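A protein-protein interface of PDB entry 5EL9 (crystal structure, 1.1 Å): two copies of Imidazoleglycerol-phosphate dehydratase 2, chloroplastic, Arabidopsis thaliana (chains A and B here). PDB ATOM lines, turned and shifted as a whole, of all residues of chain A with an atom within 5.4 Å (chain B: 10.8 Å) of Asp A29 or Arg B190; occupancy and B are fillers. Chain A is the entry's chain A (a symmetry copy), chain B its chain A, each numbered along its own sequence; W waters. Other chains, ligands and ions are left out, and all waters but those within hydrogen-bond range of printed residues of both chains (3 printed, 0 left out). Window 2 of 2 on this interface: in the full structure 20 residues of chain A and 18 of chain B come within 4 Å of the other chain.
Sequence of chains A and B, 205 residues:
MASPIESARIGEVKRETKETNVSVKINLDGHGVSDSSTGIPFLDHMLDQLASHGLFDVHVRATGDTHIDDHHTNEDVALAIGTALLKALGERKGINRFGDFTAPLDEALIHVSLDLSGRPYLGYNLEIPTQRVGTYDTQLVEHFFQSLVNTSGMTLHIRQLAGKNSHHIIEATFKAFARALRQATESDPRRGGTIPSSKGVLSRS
1 position is printed for both chains.
Of the 8 pairs that touch across the chains among the printed residues, none has its exchanged pair printed and touching as well.
Of the 15 printed residues of chain B, 3 touch a printed residue of chain A.
Of the 14 printed residues of chain A, 6 touch a printed residue of chain B.
Hydrophobic or aromatic side chains of chain A within 4 Å of the printed part of chain B: Leu A55.
The side-chain carboxylate (OD1) of Asp B188 is in salt-bridge range of the guanidinium group (NH2) of Arg A182, at 2.8 Å.
The backbone carbonyl oxygen (O) of Gly A30 sits at hydrogen-bond distance from the guanidinium group (NH2) of Arg B190 (3.0 Å).
NH1 of Arg B190 lies within salt-bridge range of OE2 of Glu A186 (2.9 Å).
The backbone NH (N) of Arg B191 lies within hydrogen-bond range of the side-chain carboxylate (OD1) of Asp B188 (3.4 Å).
The backbone carbonyl oxygen (O) of Arg A9 sits at hydrogen-bond distance from the backbone NH (N) of Leu A28.
NH2 of Arg A9 lies within salt-bridge range of OD1 of Asp A29, 2.8 Å away.
The backbone NH (N) of His A31 sits at hydrogen-bond distance from the backbone carbonyl oxygen (O) of Leu A55, 3.3 Å away.
O of Arg A182 lies within hydrogen-bond range of OG1 of Thr A185, 3.1 Å away.
The guanidinium group (NE) of Arg A182 lies within salt-bridge range of the side-chain carboxylate (OE2) of Glu A186 (3.0 Å).
Among the printed residues, pairs that only touch across the chains: Leu A28 with Arg B190, Asp A29 with Arg B190, Leu A55 with Arg B190, Leu A55 with Arg B191 and Arg A182 with Arg B190.
Water W3 lies within hydrogen-bond range of the backbone carbonyl oxygen (O) of Gly A54 (2.7 Å), the backbone carbonyl oxygen (O) of Leu A28 (2.8 Å) and the guanidinium group (NH1) of Arg B190 (2.9 Å).
Water W1 lies within hydrogen-bond range of the backbone carbonyl oxygen of Gly A30 (2.9 Å) and the guanidinium group of Arg B190 (2.9 Å).
Water W2 lies within hydrogen-bond range of the side-chain hydroxyl of Thr B194 (2.9 Å) and the backbone carbonyl oxygen of His A31 (3.3 Å).
Ala A8 touches none of the printed residues of chain B.
No residue of chain B comes within 4 Å of Arg A9.
No residue of chain B comes within 4 Å of Asn A27.
Of the printed residues of chain B, Leu A28 touches Arg B190.
Asp A29 touches one residue of chain B.
Gly A30 touches just one residue of chain B: Arg B190 (3.0 Å).
No residue of chain B comes within 4 Å of His A31.
Of the printed residues of chain B, Arg A182 touches Asp B188 (2.8 Å) and Arg B190 (3.7 Å).
Of the printed residues of chain B, Glu A186 touches Arg B190.
Of the printed residues of chain A, Asp B188 touches Arg A182.
Arg B190 touches six residues of chain A.
Of the printed residues of chain A, Arg B191 touches Leu A55.
The nearest residue of chain B that does not touch Asp A29 is Arg B191 (9.9 Å).
The nearest residue of chain A that does not touch Arg B190 is Gly A54 (4.3 Å).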
ATOM      1  N   SER A   7      -7.748 -20.041  -7.277  1.00  0.00           N
ATOM      2  CA  SER A   7      -7.762 -20.275  -5.812  1.00  0.00           C
ATOM      3  C   SER A   7      -6.570 -21.125  -5.414  1.00  0.00           C
ATOM      4  O   SER A   7      -6.105 -21.943  -6.176  1.00  0.00           O
ATOM      5  CB  SER A   7      -9.026 -21.010  -5.379  1.00  0.00           C
ATOM      6  OG  SER A   7      -9.350 -20.710  -4.033  1.00  0.00           O
ATOM      7  N   ALA A   8      -6.130 -20.946  -4.194  1.00  0.00           N
ATOM      8  CA  ALA A   8      -4.990 -21.710  -3.690  1.00  0.00           C
ATOM      9  C   ALA A   8      -5.262 -23.199  -3.654  1.00  0.00           C
ATOM     10  O   ALA A   8      -6.354 -23.638  -3.332  1.00  0.00           O
ATOM     11  CB  ALA A   8      -4.624 -21.232  -2.331  1.00  0.00           C
ATOM     12  N   ARG A   9      -4.239 -23.970  -3.992  1.00  0.00           N
ATOM     13  CA  ARG A   9      -4.338 -25.435  -3.991  1.00  0.00           C
ATOM     14  C   ARG A   9      -3.974 -25.974  -2.616  1.00  0.00           C
ATOM     15  O   ARG A   9      -2.813 -25.967  -2.220  1.00  0.00           O
ATOM     16  CB  ARG A   9      -3.408 -26.006  -5.042  1.00  0.00           C
ATOM     17  CG  ARG A   9      -3.821 -25.674  -6.467  1.00  0.00           C
ATOM     18  CD  ARG A   9      -2.697 -26.025  -7.434  1.00  0.00           C
ATOM     19  NE  ARG A   9      -1.527 -25.175  -7.182  1.00  0.00           N
ATOM     20  CZ  ARG A   9      -0.305 -25.403  -7.662  1.00  0.00           C
ATOM     21  NH1 ARG A   9      -0.043 -26.454  -8.427  1.00  0.00           N
ATOM     22  NH2 ARG A   9       0.667 -24.545  -7.355  1.00  0.00           N
ATOM     23  N   ASN A  27      -0.662 -25.963   1.720  1.00  0.00           N
ATOM     24  CA  ASN A  27      -1.019 -25.017   0.649  1.00  0.00           C
ATOM     25  C   ASN A  27       0.155 -24.922  -0.319  1.00  0.00           C
ATOM     26  O   ASN A  27       1.217 -24.428   0.066  1.00  0.00           O
ATOM     27  CB  ASN A  27      -1.348 -23.654   1.245  1.00  0.00           C
ATOM     28  CG  ASN A  27      -1.901 -22.656   0.233  1.00  0.00           C
ATOM     29  OD1 ASN A  27      -1.791 -22.819  -0.979  1.00  0.00           O
ATOM     30  ND2 ASN A  27      -2.492 -21.597   0.750  1.00  0.00           N
ATOM     31  N   LEU A  28      -0.057 -25.374  -1.548  1.00  0.00           N
ATOM     32  CA  LEU A  28       0.990 -25.299  -2.570  1.00  0.00           C
ATOM     33  C   LEU A  28       1.340 -23.874  -2.972  1.00  0.00           C
ATOM     34  O   LEU A  28       2.435 -23.615  -3.446  1.00  0.00           O
ATOM     35  CB  LEU A  28       0.595 -26.067  -3.838  1.00  0.00           C
ATOM     36  CG  LEU A  28       0.261 -27.531  -3.668  1.00  0.00           C
ATOM     37  CD1 LEU A  28      -0.086 -28.152  -5.002  1.00  0.00           C
ATOM     38  CD2 LEU A  28       1.358 -28.313  -2.968  1.00  0.00           C
ATOM     39  N   ASP A  29       0.352 -22.994  -2.811  1.00  0.00           N
ATOM     40  CA  ASP A  29       0.422 -21.595  -3.207  1.00  0.00           C
ATOM     41  C   ASP A  29       0.564 -20.707  -1.975  1.00  0.00           C
ATOM     42  O   ASP A  29       0.036 -19.611  -1.901  1.00  0.00           O
ATOM     43  CB  ASP A  29      -0.821 -21.263  -4.035  1.00  0.00           C
ATOM     44  CG  ASP A  29      -0.930 -22.144  -5.250  1.00  0.00           C
ATOM     45  OD1 ASP A  29       0.005 -22.115  -6.080  1.00  0.00           O
ATOM     46  OD2 ASP A  29      -1.929 -22.917  -5.365  1.00  0.00           O
ATOM     47  N   GLY A  30       1.360 -21.184  -1.029  1.00  0.00           N
ATOM     48  CA  GLY A  30       1.500 -20.550   0.267  1.00  0.00           C
ATOM     49  C   GLY A  30       2.447 -19.381   0.315  1.00  0.00           C
ATOM     50  O   GLY A  30       2.986 -18.908  -0.685  1.00  0.00           O
ATOM     51  N   HIS A  31       2.659 -18.944   1.549  1.00  0.00           N
ATOM     52  CA  HIS A  31       3.602 -17.864   1.865  1.00  0.00           C
ATOM     53  C   HIS A  31       4.639 -18.316   2.897  1.00  0.00           C
ATOM     54  O   HIS A  31       5.207 -17.511   3.620  1.00  0.00           O
ATOM     55  CB  HIS A  31       2.860 -16.610   2.338  1.00  0.00           C
ATOM     56  CG  HIS A  31       1.927 -16.061   1.307  1.00  0.00           C
ATOM     57  ND1 HIS A  31       0.643 -16.527   1.155  1.00  0.00           N
ATOM     58  CD2 HIS A  31       2.103 -15.120   0.347  1.00  0.00           C
ATOM     59  CE1 HIS A  31       0.050 -15.872   0.169  1.00  0.00           C
ATOM     60  NE2 HIS A  31       0.918 -15.017  -0.341  1.00  0.00           N
ATOM     61  N   GLY A  54      10.480 -23.553   0.340  1.00  0.00           N
ATOM     62  CA  GLY A  54       9.494 -23.965  -0.661  1.00  0.00           C
ATOM     63  C   GLY A  54       8.324 -23.019  -0.785  1.00  0.00           C
ATOM     64  O   GLY A  54       7.618 -23.059  -1.775  1.00  0.00           O
ATOM     65  N   LEU A  55       8.109 -22.205   0.248  1.00  0.00           N
ATOM     66  CA  LEU A  55       6.962 -21.289   0.371  1.00  0.00           C
ATOM     67  C   LEU A  55       5.620 -21.993   0.475  1.00  0.00           C
ATOM     68  O   LEU A  55       4.577 -21.351   0.463  1.00  0.00           O
ATOM     69  CB  LEU A  55       6.965 -20.184  -0.698  1.00  0.00           C
ATOM     70  CG  LEU A  55       8.145 -19.222  -0.551  1.00  0.00           C
ATOM     71  CD1 LEU A  55       8.049 -18.136  -1.606  1.00  0.00           C
ATOM     72  CD2 LEU A  55       8.324 -18.641   0.840  1.00  0.00           C
ATOM     73  N   PHE A  56       5.637 -23.287   0.738  1.00  0.00           N
ATOM     74  CA  PHE A  56       4.457 -24.005   1.140  1.00  0.00           C
ATOM     75  C   PHE A  56       3.984 -23.495   2.485  1.00  0.00           C
ATOM     76  O   PHE A  56       4.801 -23.161   3.340  1.00  0.00           O
ATOM     77  CB  PHE A  56       4.742 -25.511   1.205  1.00  0.00           C
ATOM     78  CG  PHE A  56       5.259 -26.023  -0.095  1.00  0.00           C
ATOM     79  CD1 PHE A  56       6.601 -26.295  -0.316  1.00  0.00           C
ATOM     80  CD2 PHE A  56       4.396 -26.174  -1.154  1.00  0.00           C
ATOM     81  CE1 PHE A  56       7.045 -26.690  -1.566  1.00  0.00           C
ATOM     82  CE2 PHE A  56       4.840 -26.570  -2.387  1.00  0.00           C
ATOM     83  CZ  PHE A  56       6.158 -26.821  -2.607  1.00  0.00           C
ATOM     84  N   ARG A 182       8.878 -26.724  -4.982  1.00  0.00           N
ATOM     85  CA  ARG A 182       8.324 -25.411  -5.306  1.00  0.00           C
ATOM     86  C   ARG A 182       8.305 -25.216  -6.828  1.00  0.00           C
ATOM     87  O   ARG A 182       7.279 -24.909  -7.412  1.00  0.00           O
ATOM     88  CB  ARG A 182       9.135 -24.330  -4.605  1.00  0.00           C
ATOM     89  CG  ARG A 182       8.770 -22.942  -5.061  1.00  0.00           C
ATOM     90  CD  ARG A 182       9.620 -21.921  -4.344  1.00  0.00           C
ATOM     91  NE  ARG A 182       9.361 -20.611  -4.903  1.00  0.00           N
ATOM     92  CZ  ARG A 182       9.897 -19.482  -4.447  1.00  0.00           C
ATOM     93  NH1 ARG A 182      10.686 -19.486  -3.386  1.00  0.00           N
ATOM     94  NH2 ARG A 182       9.623 -18.350  -5.063  1.00  0.00           N
ATOM     95  N   THR A 185       5.746 -27.564  -8.650  1.00  0.00           N
ATOM     96  CA  THR A 185       4.342 -27.268  -8.355  1.00  0.00           C
ATOM     97  C   THR A 185       3.882 -25.923  -8.899  1.00  0.00           C
ATOM     98  O   THR A 185       2.669 -25.711  -9.038  1.00  0.00           O
ATOM     99  CB  THR A 185       4.034 -27.330  -6.846  1.00  0.00           C
ATOM    100  OG1 THR A 185       4.781 -26.339  -6.139  1.00  0.00           O
ATOM    101  CG2 THR A 185       4.251 -28.725  -6.270  1.00  0.00           C
ATOM    102  N   GLU A 186       4.805 -25.016  -9.179  1.00  0.00           N
ATOM    103  CA  GLU A 186       4.468 -23.714  -9.679  1.00  0.00           C
ATOM    104  C   GLU A 186       3.887 -23.778 -11.093  1.00  0.00           C
ATOM    105  O   GLU A 186       4.133 -24.701 -11.868  1.00  0.00           O
ATOM    106  CB  GLU A 186       5.676 -22.766  -9.601  1.00  0.00           C
ATOM    107  CG  GLU A 186       5.895 -22.163  -8.215  1.00  0.00           C
ATOM    108  CD  GLU A 186       7.199 -21.425  -8.007  1.00  0.00           C
ATOM    109  OE1 GLU A 186       8.154 -21.662  -8.796  1.00  0.00           O
ATOM    110  OE2 GLU A 186       7.277 -20.683  -7.006  1.00  0.00           O
ATOM    111  N   LYS B  93      17.263  -9.475   2.736  1.00  0.00           N
ATOM    112  CA  LYS B  93      15.819  -9.650   2.699  1.00  0.00           C
ATOM    113  C   LYS B  93      15.297  -9.794   1.273  1.00  0.00           C
ATOM    114  O   LYS B  93      15.724  -9.086   0.370  1.00  0.00           O
ATOM    115  CB  LYS B  93      15.117  -8.527   3.414  1.00  0.00           C
ATOM    116  CG  LYS B  93      15.325  -8.592   4.926  1.00  0.00           C
ATOM    117  CD  LYS B  93      14.574  -7.482   5.632  1.00  0.00           C
ATOM    118  CE  LYS B  93      15.017  -7.250   7.055  1.00  0.00           C
ATOM    119  NZ  LYS B  93      13.911  -6.624   7.820  1.00  0.00           N
ATOM    120  N   GLY B  94      14.365 -10.717   1.100  1.00  0.00           N
ATOM    121  CA  GLY B  94      13.633 -10.828  -0.150  1.00  0.00           C
ATOM    122  C   GLY B  94      14.329 -11.508  -1.316  1.00  0.00           C
ATOM    123  O   GLY B  94      13.786 -11.520  -2.406  1.00  0.00           O
ATOM    124  N   ILE B  95      15.516 -12.060  -1.095  1.00  0.00           N
ATOM    125  CA  ILE B  95      16.321 -12.638  -2.165  1.00  0.00           C
ATOM    126  C   ILE B  95      16.084 -14.133  -2.288  1.00  0.00           C
ATOM    127  O   ILE B  95      15.626 -14.804  -1.363  1.00  0.00           O
ATOM    128  CB  ILE B  95      17.838 -12.333  -1.995  1.00  0.00           C
ATOM    129  CG1 ILE B  95      18.470 -13.037  -0.796  1.00  0.00           C
ATOM    130  CG2 ILE B  95      18.062 -10.834  -1.989  1.00  0.00           C
ATOM    131  CD1 ILE B  95      19.970 -12.942  -0.727  1.00  0.00           C
ATOM    132  N   ASN B  96      16.488 -14.665  -3.442  1.00  0.00           N
ATOM    133  CA  ASN B  96      16.425 -16.104  -3.663  1.00  0.00           C
ATOM    134  C   ASN B  96      17.358 -16.868  -2.743  1.00  0.00           C
ATOM    135  O   ASN B  96      17.049 -18.020  -2.418  1.00  0.00           O
ATOM    136  CB  ASN B  96      16.793 -16.432  -5.113  1.00  0.00           C
ATOM    137  CG  ASN B  96      15.672 -16.144  -6.081  1.00  0.00           C
ATOM    138  OD1 ASN B  96      14.483 -16.287  -5.756  1.00  0.00           O
ATOM    139  ND2 ASN B  96      16.049 -15.744  -7.287  1.00  0.00           N
ATOM    140  N   GLU B 186      19.126 -12.262  -6.922  1.00  0.00           N
ATOM    141  CA  GLU B 186      17.896 -11.732  -7.440  1.00  0.00           C
ATOM    142  C   GLU B 186      16.757 -11.840  -6.425  1.00  0.00           C
ATOM    143  O   GLU B 186      16.746 -12.682  -5.528  1.00  0.00           O
ATOM    144  CB  GLU B 186      17.533 -12.395  -8.778  1.00  0.00           C
ATOM    145  CG  GLU B 186      18.275 -11.807  -9.977  1.00  0.00           C
ATOM    146  CD  GLU B 186      18.153 -12.570 -11.277  1.00  0.00           C
ATOM    147  OE1 GLU B 186      17.803 -13.781 -11.230  1.00  0.00           O
ATOM    148  OE2 GLU B 186      18.491 -11.972 -12.319  1.00  0.00           O
ATOM    149  N   SER B 187      15.759 -10.989  -6.632  1.00  0.00           N
ATOM    150  CA  SER B 187      14.537 -11.010  -5.835  1.00  0.00           C
ATOM    151  C   SER B 187      13.784 -12.331  -5.974  1.00  0.00           C
ATOM    152  O   SER B 187      13.622 -12.848  -7.079  1.00  0.00           O
ATOM    153  CB  SER B 187      13.606  -9.887  -6.287  1.00  0.00           C
ATOM    154  OG  SER B 187      12.449  -9.851  -5.509  1.00  0.00           O
ATOM    155  N   ASP B 188      13.282 -12.841  -4.859  1.00  0.00           N
ATOM    156  CA  ASP B 188      12.372 -13.984  -4.864  1.00  0.00           C
ATOM    157  C   ASP B 188      10.979 -13.370  -5.007  1.00  0.00           C
ATOM    158  O   ASP B 188      10.530 -12.669  -4.118  1.00  0.00           O
ATOM    159  CB  ASP B 188      12.508 -14.775  -3.572  1.00  0.00           C
ATOM    160  CG  ASP B 188      11.550 -15.944  -3.474  1.00  0.00           C
ATOM    161  OD1 ASP B 188      10.443 -15.853  -4.069  1.00  0.00           O
ATOM    162  OD2 ASP B 188      11.893 -16.955  -2.835  1.00  0.00           O
ATOM    163  N   PRO B 189      10.290 -13.627  -6.138  1.00  0.00           N
ATOM    164  CA  PRO B 189       9.027 -12.925  -6.388  1.00  0.00           C
ATOM    165  C   PRO B 189       7.862 -13.303  -5.499  1.00  0.00           C
ATOM    166  O   PRO B 189       6.834 -12.636  -5.538  1.00  0.00           O
ATOM    167  CB  PRO B 189       8.705 -13.298  -7.835  1.00  0.00           C
ATOM    168  CG  PRO B 189       9.321 -14.643  -7.999  1.00  0.00           C
ATOM    169  CD  PRO B 189      10.606 -14.565  -7.223  1.00  0.00           C
ATOM    170  N   ARG B 190       8.013 -14.357  -4.719  1.00  0.00           N
ATOM    171  CA  ARG B 190       6.936 -14.786  -3.865  1.00  0.00           C
ATOM    172  C   ARG B 190       7.119 -14.508  -2.400  1.00  0.00           C
ATOM    173  O   ARG B 190       6.173 -14.611  -1.644  1.00  0.00           O
ATOM    174  CB  ARG B 190       6.698 -16.272  -4.021  1.00  0.00           C
ATOM    175  CG  ARG B 190       5.953 -16.615  -5.281  1.00  0.00           C
ATOM    176  CD  ARG B 190       5.755 -18.114  -5.414  1.00  0.00           C
ATOM    177  NE  ARG B 190       4.914 -18.660  -4.345  1.00  0.00           N
ATOM    178  CZ  ARG B 190       4.813 -19.957  -4.057  1.00  0.00           C
ATOM    179  NH1 ARG B 190       5.478 -20.862  -4.750  1.00  0.00           N
ATOM    180  NH2 ARG B 190       4.020 -20.338  -3.067  1.00  0.00           N
ATOM    181  N   ARG B 191       8.320 -14.194  -1.949  1.00  0.00           N
ATOM    182  CA  ARG B 191       8.513 -14.166  -0.486  1.00  0.00           C
ATOM    183  C   ARG B 191       8.261 -12.875   0.265  1.00  0.00           C
ATOM    184  O   ARG B 191       8.457 -12.780   1.476  1.00  0.00           O
ATOM    185  CB  ARG B 191       9.785 -14.802  -0.075  1.00  0.00           C
ATOM    186  CG  ARG B 191      11.003 -13.924  -0.194  1.00  0.00           C
ATOM    187  CD  ARG B 191      12.213 -14.676   0.399  1.00  0.00           C
ATOM    188  NE  ARG B 191      11.818 -15.355   1.651  1.00  0.00           N
ATOM    189  CZ  ARG B 191      11.745 -16.688   1.911  1.00  0.00           C
ATOM    190  NH1 ARG B 191      11.226 -17.114   3.047  1.00  0.00           N
ATOM    191  NH2 ARG B 191      12.204 -17.606   1.101  1.00  0.00           N
ATOM    192  N   GLY B 192       7.780 -11.894  -0.449  1.00  0.00           N
ATOM    193  CA  GLY B 192       7.305 -10.679   0.168  1.00  0.00           C
ATOM    194  C   GLY B 192       8.285  -9.911   0.989  1.00  0.00           C
ATOM    195  O   GLY B 192       7.915  -9.312   1.990  1.00  0.00           O
ATOM    196  N   GLY B 193       9.522  -9.892   0.544  1.00  0.00           N
ATOM    197  CA  GLY B 193      10.563  -9.174   1.247  1.00  0.00           C
ATOM    198  C   GLY B 193      11.038  -9.760   2.577  1.00  0.00           C
ATOM    199  O   GLY B 193      11.807  -9.117   3.260  1.00  0.00           O
ATOM    200  N   THR B 194      10.599 -10.942   2.935  1.00  0.00           N
ATOM    201  CA  THR B 194      11.037 -11.543   4.189  1.00  0.00           C
ATOM    202  C   THR B 194      12.483 -12.042   4.091  1.00  0.00           C
ATOM    203  O   THR B 194      12.977 -12.320   3.000  1.00  0.00           O
ATOM    204  CB  THR B 194      10.088 -12.723   4.569  1.00  0.00           C
ATOM    205  OG1 THR B 194      10.133 -13.758   3.571  1.00  0.00           O
ATOM    206  CG2 THR B 194       8.652 -12.229   4.783  1.00  0.00           C
ATOM    207  N   ILE B 195      13.136 -12.222   5.230  1.00  0.00           N
ATOM    208  CA  ILE B 195      14.453 -12.869   5.287  1.00  0.00           C
ATOM    209  C   ILE B 195      14.305 -14.339   4.917  1.00  0.00           C
ATOM    210  O   ILE B 195      13.512 -15.026   5.530  1.00  0.00           O
ATOM    211  CB  ILE B 195      15.045 -12.794   6.718  1.00  0.00           C
ATOM    212  CG1 ILE B 195      16.485 -13.300   6.732  1.00  0.00           C
ATOM    213  CG2 ILE B 195      14.159 -13.521   7.767  1.00  0.00           C
ATOM    214  CD1 ILE B 195      17.459 -12.253   6.293  1.00  0.00           C
ATOM    215  N   PRO B 196      15.108 -14.845   3.973  1.00  0.00           N
ATOM    216  CA  PRO B 196      14.945 -16.246   3.579  1.00  0.00           C
ATOM    217  C   PRO B 196      15.744 -17.184   4.498  1.00  0.00           C
ATOM    218  O   PRO B 196      16.696 -17.819   4.073  1.00  0.00           O
ATOM    219  CB  PRO B 196      15.474 -16.258   2.142  1.00  0.00           C
ATOM    220  CG  PRO B 196      16.521 -15.174   2.145  1.00  0.00           C
ATOM    221  CD  PRO B 196      15.968 -14.105   3.048  1.00  0.00           C
HETATM  222  O   HOH W   1       3.032 -17.028  -2.865  1.00  0.00           O
HETATM  223  O   HOH W   2       7.904 -15.664   3.460  1.00  0.00           O
HETATM  224  O   HOH W   3       5.203 -23.125  -3.017  1.00  0.00           O
